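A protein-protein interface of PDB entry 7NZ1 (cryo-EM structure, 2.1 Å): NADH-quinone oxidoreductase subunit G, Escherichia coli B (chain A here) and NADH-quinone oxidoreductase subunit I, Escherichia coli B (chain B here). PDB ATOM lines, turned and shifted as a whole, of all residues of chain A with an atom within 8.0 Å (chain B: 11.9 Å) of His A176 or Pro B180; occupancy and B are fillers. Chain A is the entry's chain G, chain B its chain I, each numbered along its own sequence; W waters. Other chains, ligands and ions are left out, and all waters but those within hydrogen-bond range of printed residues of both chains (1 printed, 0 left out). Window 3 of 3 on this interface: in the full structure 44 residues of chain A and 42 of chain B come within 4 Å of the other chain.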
ATOM      1  N   ALA A 153       3.325 -11.798  -9.131  1.00  0.00           N
ATOM      2  CA  ALA A 153       2.214 -10.933  -8.695  1.00  0.00           C
ATOM      3  C   ALA A 153       2.408  -9.478  -9.125  1.00  0.00           C
ATOM      4  O   ALA A 153       2.273  -8.548  -8.335  1.00  0.00           O
ATOM      5  CB  ALA A 153       1.971 -11.039  -7.184  1.00  0.00           C
ATOM      6  N   TYR A 155       0.550  -8.118 -11.528  1.00  0.00           N
ATOM      7  CA  TYR A 155      -0.817  -7.736 -11.901  1.00  0.00           C
ATOM      8  C   TYR A 155      -0.938  -7.247 -13.338  1.00  0.00           C
ATOM      9  O   TYR A 155      -1.964  -6.665 -13.681  1.00  0.00           O
ATOM     10  CB  TYR A 155      -1.430  -6.674 -10.963  1.00  0.00           C
ATOM     11  CG  TYR A 155      -1.681  -7.147  -9.546  1.00  0.00           C
ATOM     12  CD1 TYR A 155      -0.633  -7.280  -8.642  1.00  0.00           C
ATOM     13  CD2 TYR A 155      -2.966  -7.459  -9.112  1.00  0.00           C
ATOM     14  CE1 TYR A 155      -0.847  -7.716  -7.353  1.00  0.00           C
ATOM     15  CE2 TYR A 155      -3.192  -7.902  -7.819  1.00  0.00           C
ATOM     16  CZ  TYR A 155      -2.126  -8.030  -6.947  1.00  0.00           C
ATOM     17  OH  TYR A 155      -2.330  -8.459  -5.661  1.00  0.00           O
ATOM     18  N   TYR A 173      -7.389 -13.899  -7.412  1.00  0.00           N
ATOM     19  CA  TYR A 173      -8.083 -14.570  -6.322  1.00  0.00           C
ATOM     20  C   TYR A 173      -7.158 -14.663  -5.120  1.00  0.00           C
ATOM     21  O   TYR A 173      -5.936 -14.626  -5.251  1.00  0.00           O
ATOM     22  CB  TYR A 173      -8.539 -15.971  -6.754  1.00  0.00           C
ATOM     23  CG  TYR A 173      -9.135 -15.932  -8.130  1.00  0.00           C
ATOM     24  CD1 TYR A 173     -10.341 -15.281  -8.367  1.00  0.00           C
ATOM     25  CD2 TYR A 173      -8.439 -16.452  -9.215  1.00  0.00           C
ATOM     26  CE1 TYR A 173     -10.865 -15.203  -9.638  1.00  0.00           C
ATOM     27  CE2 TYR A 173      -8.954 -16.378 -10.488  1.00  0.00           C
ATOM     28  CZ  TYR A 173     -10.164 -15.751 -10.694  1.00  0.00           C
ATOM     29  OH  TYR A 173     -10.669 -15.680 -11.964  1.00  0.00           O
ATOM     30  N   GLY A 174      -7.756 -14.799  -3.946  1.00  0.00           N
ATOM     31  CA  GLY A 174      -6.996 -14.990  -2.729  1.00  0.00           C
ATOM     32  C   GLY A 174      -6.581 -13.678  -2.092  1.00  0.00           C
ATOM     33  O   GLY A 174      -7.122 -12.608  -2.373  1.00  0.00           O
ATOM     34  N   ALA A 175      -5.570 -13.775  -1.234  1.00  0.00           N
ATOM     35  CA  ALA A 175      -5.040 -12.632  -0.498  1.00  0.00           C
ATOM     36  C   ALA A 175      -3.633 -12.976  -0.037  1.00  0.00           C
ATOM     37  O   ALA A 175      -3.201 -14.127  -0.133  1.00  0.00           O
ATOM     38  CB  ALA A 175      -5.925 -12.256   0.692  1.00  0.00           C
ATOM     39  N   HIS A 176      -2.933 -11.948   0.470  1.00  0.00           N
ATOM     40  CA  HIS A 176      -1.551 -11.931   1.035  1.00  0.00           C
ATOM     41  C   HIS A 176      -0.615 -12.593   0.023  1.00  0.00           C
ATOM     42  O   HIS A 176      -0.645 -12.221  -1.158  1.00  0.00           O
ATOM     43  CB  HIS A 176      -1.459 -12.474   2.481  1.00  0.00           C
ATOM     44  CG  HIS A 176      -2.150 -13.781   2.731  1.00  0.00           C
ATOM     45  ND1 HIS A 176      -1.528 -14.999   2.562  1.00  0.00           N
ATOM     46  CD2 HIS A 176      -3.409 -14.059   3.146  1.00  0.00           C
ATOM     47  CE1 HIS A 176      -2.373 -15.969   2.858  1.00  0.00           C
ATOM     48  NE2 HIS A 176      -3.522 -15.424   3.214  1.00  0.00           N
ATOM     49  N   ASP A 177       0.196 -13.564   0.420  1.00  0.00           N
ATOM     50  CA  ASP A 177       1.160 -14.196  -0.464  1.00  0.00           C
ATOM     51  C   ASP A 177       0.587 -15.391  -1.220  1.00  0.00           C
ATOM     52  O   ASP A 177       1.337 -16.095  -1.901  1.00  0.00           O
ATOM     53  CB  ASP A 177       2.409 -14.590   0.332  1.00  0.00           C
ATOM     54  CG  ASP A 177       2.204 -15.823   1.187  1.00  0.00           C
ATOM     55  OD1 ASP A 177       1.183 -15.891   1.899  1.00  0.00           O
ATOM     56  OD2 ASP A 177       3.070 -16.722   1.157  1.00  0.00           O
ATOM     57  N   ASN A 178      -0.722 -15.626  -1.120  1.00  0.00           N
ATOM     58  CA  ASN A 178      -1.394 -16.726  -1.796  1.00  0.00           C
ATOM     59  C   ASN A 178      -2.219 -16.259  -3.006  1.00  0.00           C
ATOM     60  O   ASN A 178      -3.153 -16.954  -3.413  1.00  0.00           O
ATOM     61  CB  ASN A 178      -2.255 -17.502  -0.793  1.00  0.00           C
ATOM     62  CG  ASN A 178      -2.494 -18.949  -1.216  1.00  0.00           C
ATOM     63  OD1 ASN A 178      -1.550 -19.694  -1.454  1.00  0.00           O
ATOM     64  ND2 ASN A 178      -3.755 -19.346  -1.297  1.00  0.00           N
ATOM     65  N   VAL A 179      -1.940 -15.056  -3.529  1.00  0.00           N
ATOM     66  CA  VAL A 179      -2.693 -14.506  -4.660  1.00  0.00           C
ATOM     67  C   VAL A 179      -2.537 -15.376  -5.906  1.00  0.00           C
ATOM     68  O   VAL A 179      -1.437 -15.832  -6.241  1.00  0.00           O
ATOM     69  CB  VAL A 179      -2.285 -13.048  -4.937  1.00  0.00           C
ATOM     70  CG1 VAL A 179      -2.923 -12.120  -3.928  1.00  0.00           C
ATOM     71  CG2 VAL A 179      -0.779 -12.874  -4.929  1.00  0.00           C
ATOM     72  N   TYR A 180      -3.657 -15.634  -6.580  1.00  0.00           N
ATOM     73  CA  TYR A 180      -3.730 -16.543  -7.715  1.00  0.00           C
ATOM     74  C   TYR A 180      -4.341 -15.812  -8.901  1.00  0.00           C
ATOM     75  O   TYR A 180      -5.415 -15.218  -8.784  1.00  0.00           O
ATOM     76  CB  TYR A 180      -4.553 -17.793  -7.353  1.00  0.00           C
ATOM     77  CG  TYR A 180      -4.493 -18.958  -8.322  1.00  0.00           C
ATOM     78  CD1 TYR A 180      -5.274 -18.990  -9.479  1.00  0.00           C
ATOM     79  CD2 TYR A 180      -3.656 -20.037  -8.070  1.00  0.00           C
ATOM     80  CE1 TYR A 180      -5.213 -20.064 -10.355  1.00  0.00           C
ATOM     81  CE2 TYR A 180      -3.591 -21.110  -8.932  1.00  0.00           C
ATOM     82  CZ  TYR A 180      -4.366 -21.119 -10.072  1.00  0.00           C
ATOM     83  OH  TYR A 180      -4.286 -22.193 -10.919  1.00  0.00           O
ATOM     84  N   LYS B 171       3.253 -27.547   0.464  1.00  0.00           N
ATOM     85  CA  LYS B 171       2.050 -28.021  -0.202  1.00  0.00           C
ATOM     86  C   LYS B 171       1.264 -26.853  -0.799  1.00  0.00           C
ATOM     87  O   LYS B 171       1.261 -25.753  -0.241  1.00  0.00           O
ATOM     88  CB  LYS B 171       1.160 -28.773   0.784  1.00  0.00           C
ATOM     89  CG  LYS B 171       1.657 -30.135   1.176  1.00  0.00           C
ATOM     90  CD  LYS B 171       1.787 -31.033  -0.028  1.00  0.00           C
ATOM     91  CE  LYS B 171       3.157 -31.663  -0.069  1.00  0.00           C
ATOM     92  NZ  LYS B 171       3.393 -32.539   1.111  1.00  0.00           N
ATOM     93  N   PRO B 172       0.599 -27.063  -1.939  1.00  0.00           N
ATOM     94  CA  PRO B 172      -0.238 -25.996  -2.513  1.00  0.00           C
ATOM     95  C   PRO B 172      -1.467 -25.729  -1.651  1.00  0.00           C
ATOM     96  O   PRO B 172      -2.177 -26.652  -1.251  1.00  0.00           O
ATOM     97  CB  PRO B 172      -0.632 -26.543  -3.891  1.00  0.00           C
ATOM     98  CG  PRO B 172       0.230 -27.717  -4.129  1.00  0.00           C
ATOM     99  CD  PRO B 172       0.648 -28.251  -2.807  1.00  0.00           C
ATOM    100  N   ILE B 173      -1.711 -24.452  -1.373  1.00  0.00           N
ATOM    101  CA  ILE B 173      -2.889 -24.006  -0.639  1.00  0.00           C
ATOM    102  C   ILE B 173      -3.854 -23.374  -1.626  1.00  0.00           C
ATOM    103  O   ILE B 173      -3.491 -22.439  -2.349  1.00  0.00           O
ATOM    104  CB  ILE B 173      -2.524 -23.009   0.475  1.00  0.00           C
ATOM    105  CG1 ILE B 173      -1.291 -23.495   1.240  1.00  0.00           C
ATOM    106  CG2 ILE B 173      -3.732 -22.745   1.374  1.00  0.00           C
ATOM    107  CD1 ILE B 173      -0.997 -22.736   2.508  1.00  0.00           C
ATOM    108  N   ASP B 174      -5.085 -23.871  -1.645  1.00  0.00           N
ATOM    109  CA  ASP B 174      -6.090 -23.321  -2.535  1.00  0.00           C
ATOM    110  C   ASP B 174      -6.568 -21.976  -2.001  1.00  0.00           C
ATOM    111  O   ASP B 174      -6.557 -21.726  -0.794  1.00  0.00           O
ATOM    112  CB  ASP B 174      -7.264 -24.289  -2.666  1.00  0.00           C
ATOM    113  CG  ASP B 174      -8.093 -24.048  -3.919  1.00  0.00           C
ATOM    114  OD1 ASP B 174      -8.726 -22.983  -4.041  1.00  0.00           O
ATOM    115  OD2 ASP B 174      -8.114 -24.948  -4.783  1.00  0.00           O
ATOM    116  N   VAL B 175      -7.008 -21.112  -2.920  1.00  0.00           N
ATOM    117  CA  VAL B 175      -7.587 -19.829  -2.539  1.00  0.00           C
ATOM    118  C   VAL B 175      -8.915 -19.992  -1.808  1.00  0.00           C
ATOM    119  O   VAL B 175      -9.330 -19.082  -1.083  1.00  0.00           O
ATOM    120  CB  VAL B 175      -7.741 -18.923  -3.773  1.00  0.00           C
ATOM    121  CG1 VAL B 175      -6.391 -18.361  -4.166  1.00  0.00           C
ATOM    122  CG2 VAL B 175      -8.349 -19.691  -4.928  1.00  0.00           C
ATOM    123  N   LYS B 176      -9.598 -21.119  -1.989  1.00  0.00           N
ATOM    124  CA  LYS B 176     -10.883 -21.369  -1.351  1.00  0.00           C
ATOM    125  C   LYS B 176     -10.748 -21.922   0.064  1.00  0.00           C
ATOM    126  O   LYS B 176     -11.778 -22.179   0.699  1.00  0.00           O
ATOM    127  CB  LYS B 176     -11.710 -22.340  -2.200  1.00  0.00           C
ATOM    128  CG  LYS B 176     -11.898 -21.908  -3.644  1.00  0.00           C
ATOM    129  CD  LYS B 176     -13.033 -22.665  -4.317  1.00  0.00           C
ATOM    130  CE  LYS B 176     -12.828 -24.173  -4.294  1.00  0.00           C
ATOM    131  NZ  LYS B 176     -11.510 -24.598  -4.835  1.00  0.00           N
ATOM    132  N   SER B 177      -9.517 -22.142   0.543  1.00  0.00           N
ATOM    133  CA  SER B 177      -9.268 -22.690   1.876  1.00  0.00           C
ATOM    134  C   SER B 177      -9.828 -21.806   2.988  1.00  0.00           C
ATOM    135  O   SER B 177      -9.818 -20.575   2.898  1.00  0.00           O
ATOM    136  CB  SER B 177      -7.770 -22.901   2.094  1.00  0.00           C
ATOM    137  OG  SER B 177      -7.065 -21.675   2.051  1.00  0.00           O
ATOM    138  N   LEU B 178     -10.349 -22.458   4.033  1.00  0.00           N
ATOM    139  CA  LEU B 178     -11.004 -21.744   5.125  1.00  0.00           C
ATOM    140  C   LEU B 178     -10.013 -20.977   5.988  1.00  0.00           C
ATOM    141  O   LEU B 178     -10.383 -19.970   6.600  1.00  0.00           O
ATOM    142  CB  LEU B 178     -11.793 -22.720   5.995  1.00  0.00           C
ATOM    143  CG  LEU B 178     -12.914 -23.481   5.290  1.00  0.00           C
ATOM    144  CD1 LEU B 178     -13.321 -24.714   6.076  1.00  0.00           C
ATOM    145  CD2 LEU B 178     -14.097 -22.572   5.039  1.00  0.00           C
ATOM    146  N   LEU B 179      -8.774 -21.445   6.067  1.00  0.00           N
ATOM    147  CA  LEU B 179      -7.785 -20.810   6.929  1.00  0.00           C
ATOM    148  C   LEU B 179      -7.330 -19.494   6.310  1.00  0.00           C
ATOM    149  O   LEU B 179      -7.058 -19.445   5.106  1.00  0.00           O
ATOM    150  CB  LEU B 179      -6.579 -21.722   7.142  1.00  0.00           C
ATOM    151  CG  LEU B 179      -6.771 -22.983   7.986  1.00  0.00           C
ATOM    152  CD1 LEU B 179      -5.716 -24.009   7.628  1.00  0.00           C
ATOM    153  CD2 LEU B 179      -6.741 -22.668   9.471  1.00  0.00           C
ATOM    154  N   PRO B 180      -7.254 -18.405   7.088  1.00  0.00           N
ATOM    155  CA  PRO B 180      -6.763 -17.117   6.593  1.00  0.00           C
ATOM    156  C   PRO B 180      -5.238 -17.017   6.601  1.00  0.00           C
ATOM    157  O   PRO B 180      -4.567 -17.924   6.112  1.00  0.00           O
ATOM    158  CB  PRO B 180      -7.380 -16.122   7.570  1.00  0.00           C
ATOM    159  CG  PRO B 180      -7.435 -16.872   8.852  1.00  0.00           C
ATOM    160  CD  PRO B 180      -7.701 -18.315   8.491  1.00  0.00           C
HETATM  161  O   HOH W   1      -0.162 -22.072  -2.415  1.00  0.00           O
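Of chain B, only Pro B180 comes within 4 Å of His A176. Of chain A, only His A176 (3.97 Å) comes within 4 Å of Pro B180. Gly A174 touches just one residue of chain B: Val B175 (3.7 Å). No residue of chain B comes within 4 Å of Ala A175. No residue of chain B comes within 4 Å of Asp A177. Of chain B, only Ile B173 (3.3 Å), Asp B174 (3.7 Å) and Val B175 (3.6 Å) come within 4 Å of Asn A178. No residue of chain B comes within 4 Å of Val A179. Of the printed residues of chain A, Asp B174 touches Asn A178 (3.7 Å). Printed residues of chain B within 4 Å of Tyr A173: Val B175. Printed residues of chain A within 4 Å of Ile B173: Asn A178. Printed residues of chain B within 4 Å of Tyr A180: Val B175 (3.7 Å). Printed residues of chain A within 4 Å of Val B175: Tyr A173, Gly A174, Asn A178 and Tyr A180. The nearest printed residue of chain B that does not touch Tyr A180 is Ile B173 (6.2 Å).
Water W1 bridges OD1 of Asn A178 (2.9 Å) and N of Ile B173 (3.0 Å).
Of the 10 printed residues of chain B, 4 touch a printed residue of chain A. Hydrophobic or aromatic side chains of chain B that line the printed part of chain A: Ile B173 and Val B175. Among the printed residues, 7 pairs touch across the chains.
The side-chain amide nitrogen of Asn A178 lies within hydrogen-bond range of the backbone carbonyl oxygen of Ile B173 (3.3 Å).
Among the printed residues, merely in contact across the chains: Tyr A173 with Val B175, Gly A174 with Val B175, His A176 with Pro B180, Asn A178 with Asp B174, Asn A178 with Val B175 and Tyr A180 with Val B175.
O of Tyr A180 is in hydrogen-bond range of N of Tyr A173, 2.7 Å away. ND1 of His A176 is in hydrogen-bond range of OD1 of Asp A177 (2.9 Å). The side-chain carboxylate (OD1) of Asp B174 lies within salt-bridge range of the side-chain amino group (NZ) of Lys B176 (3.3 Å). O of Asp B174 lies within hydrogen-bond range of OG of Ser B177.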
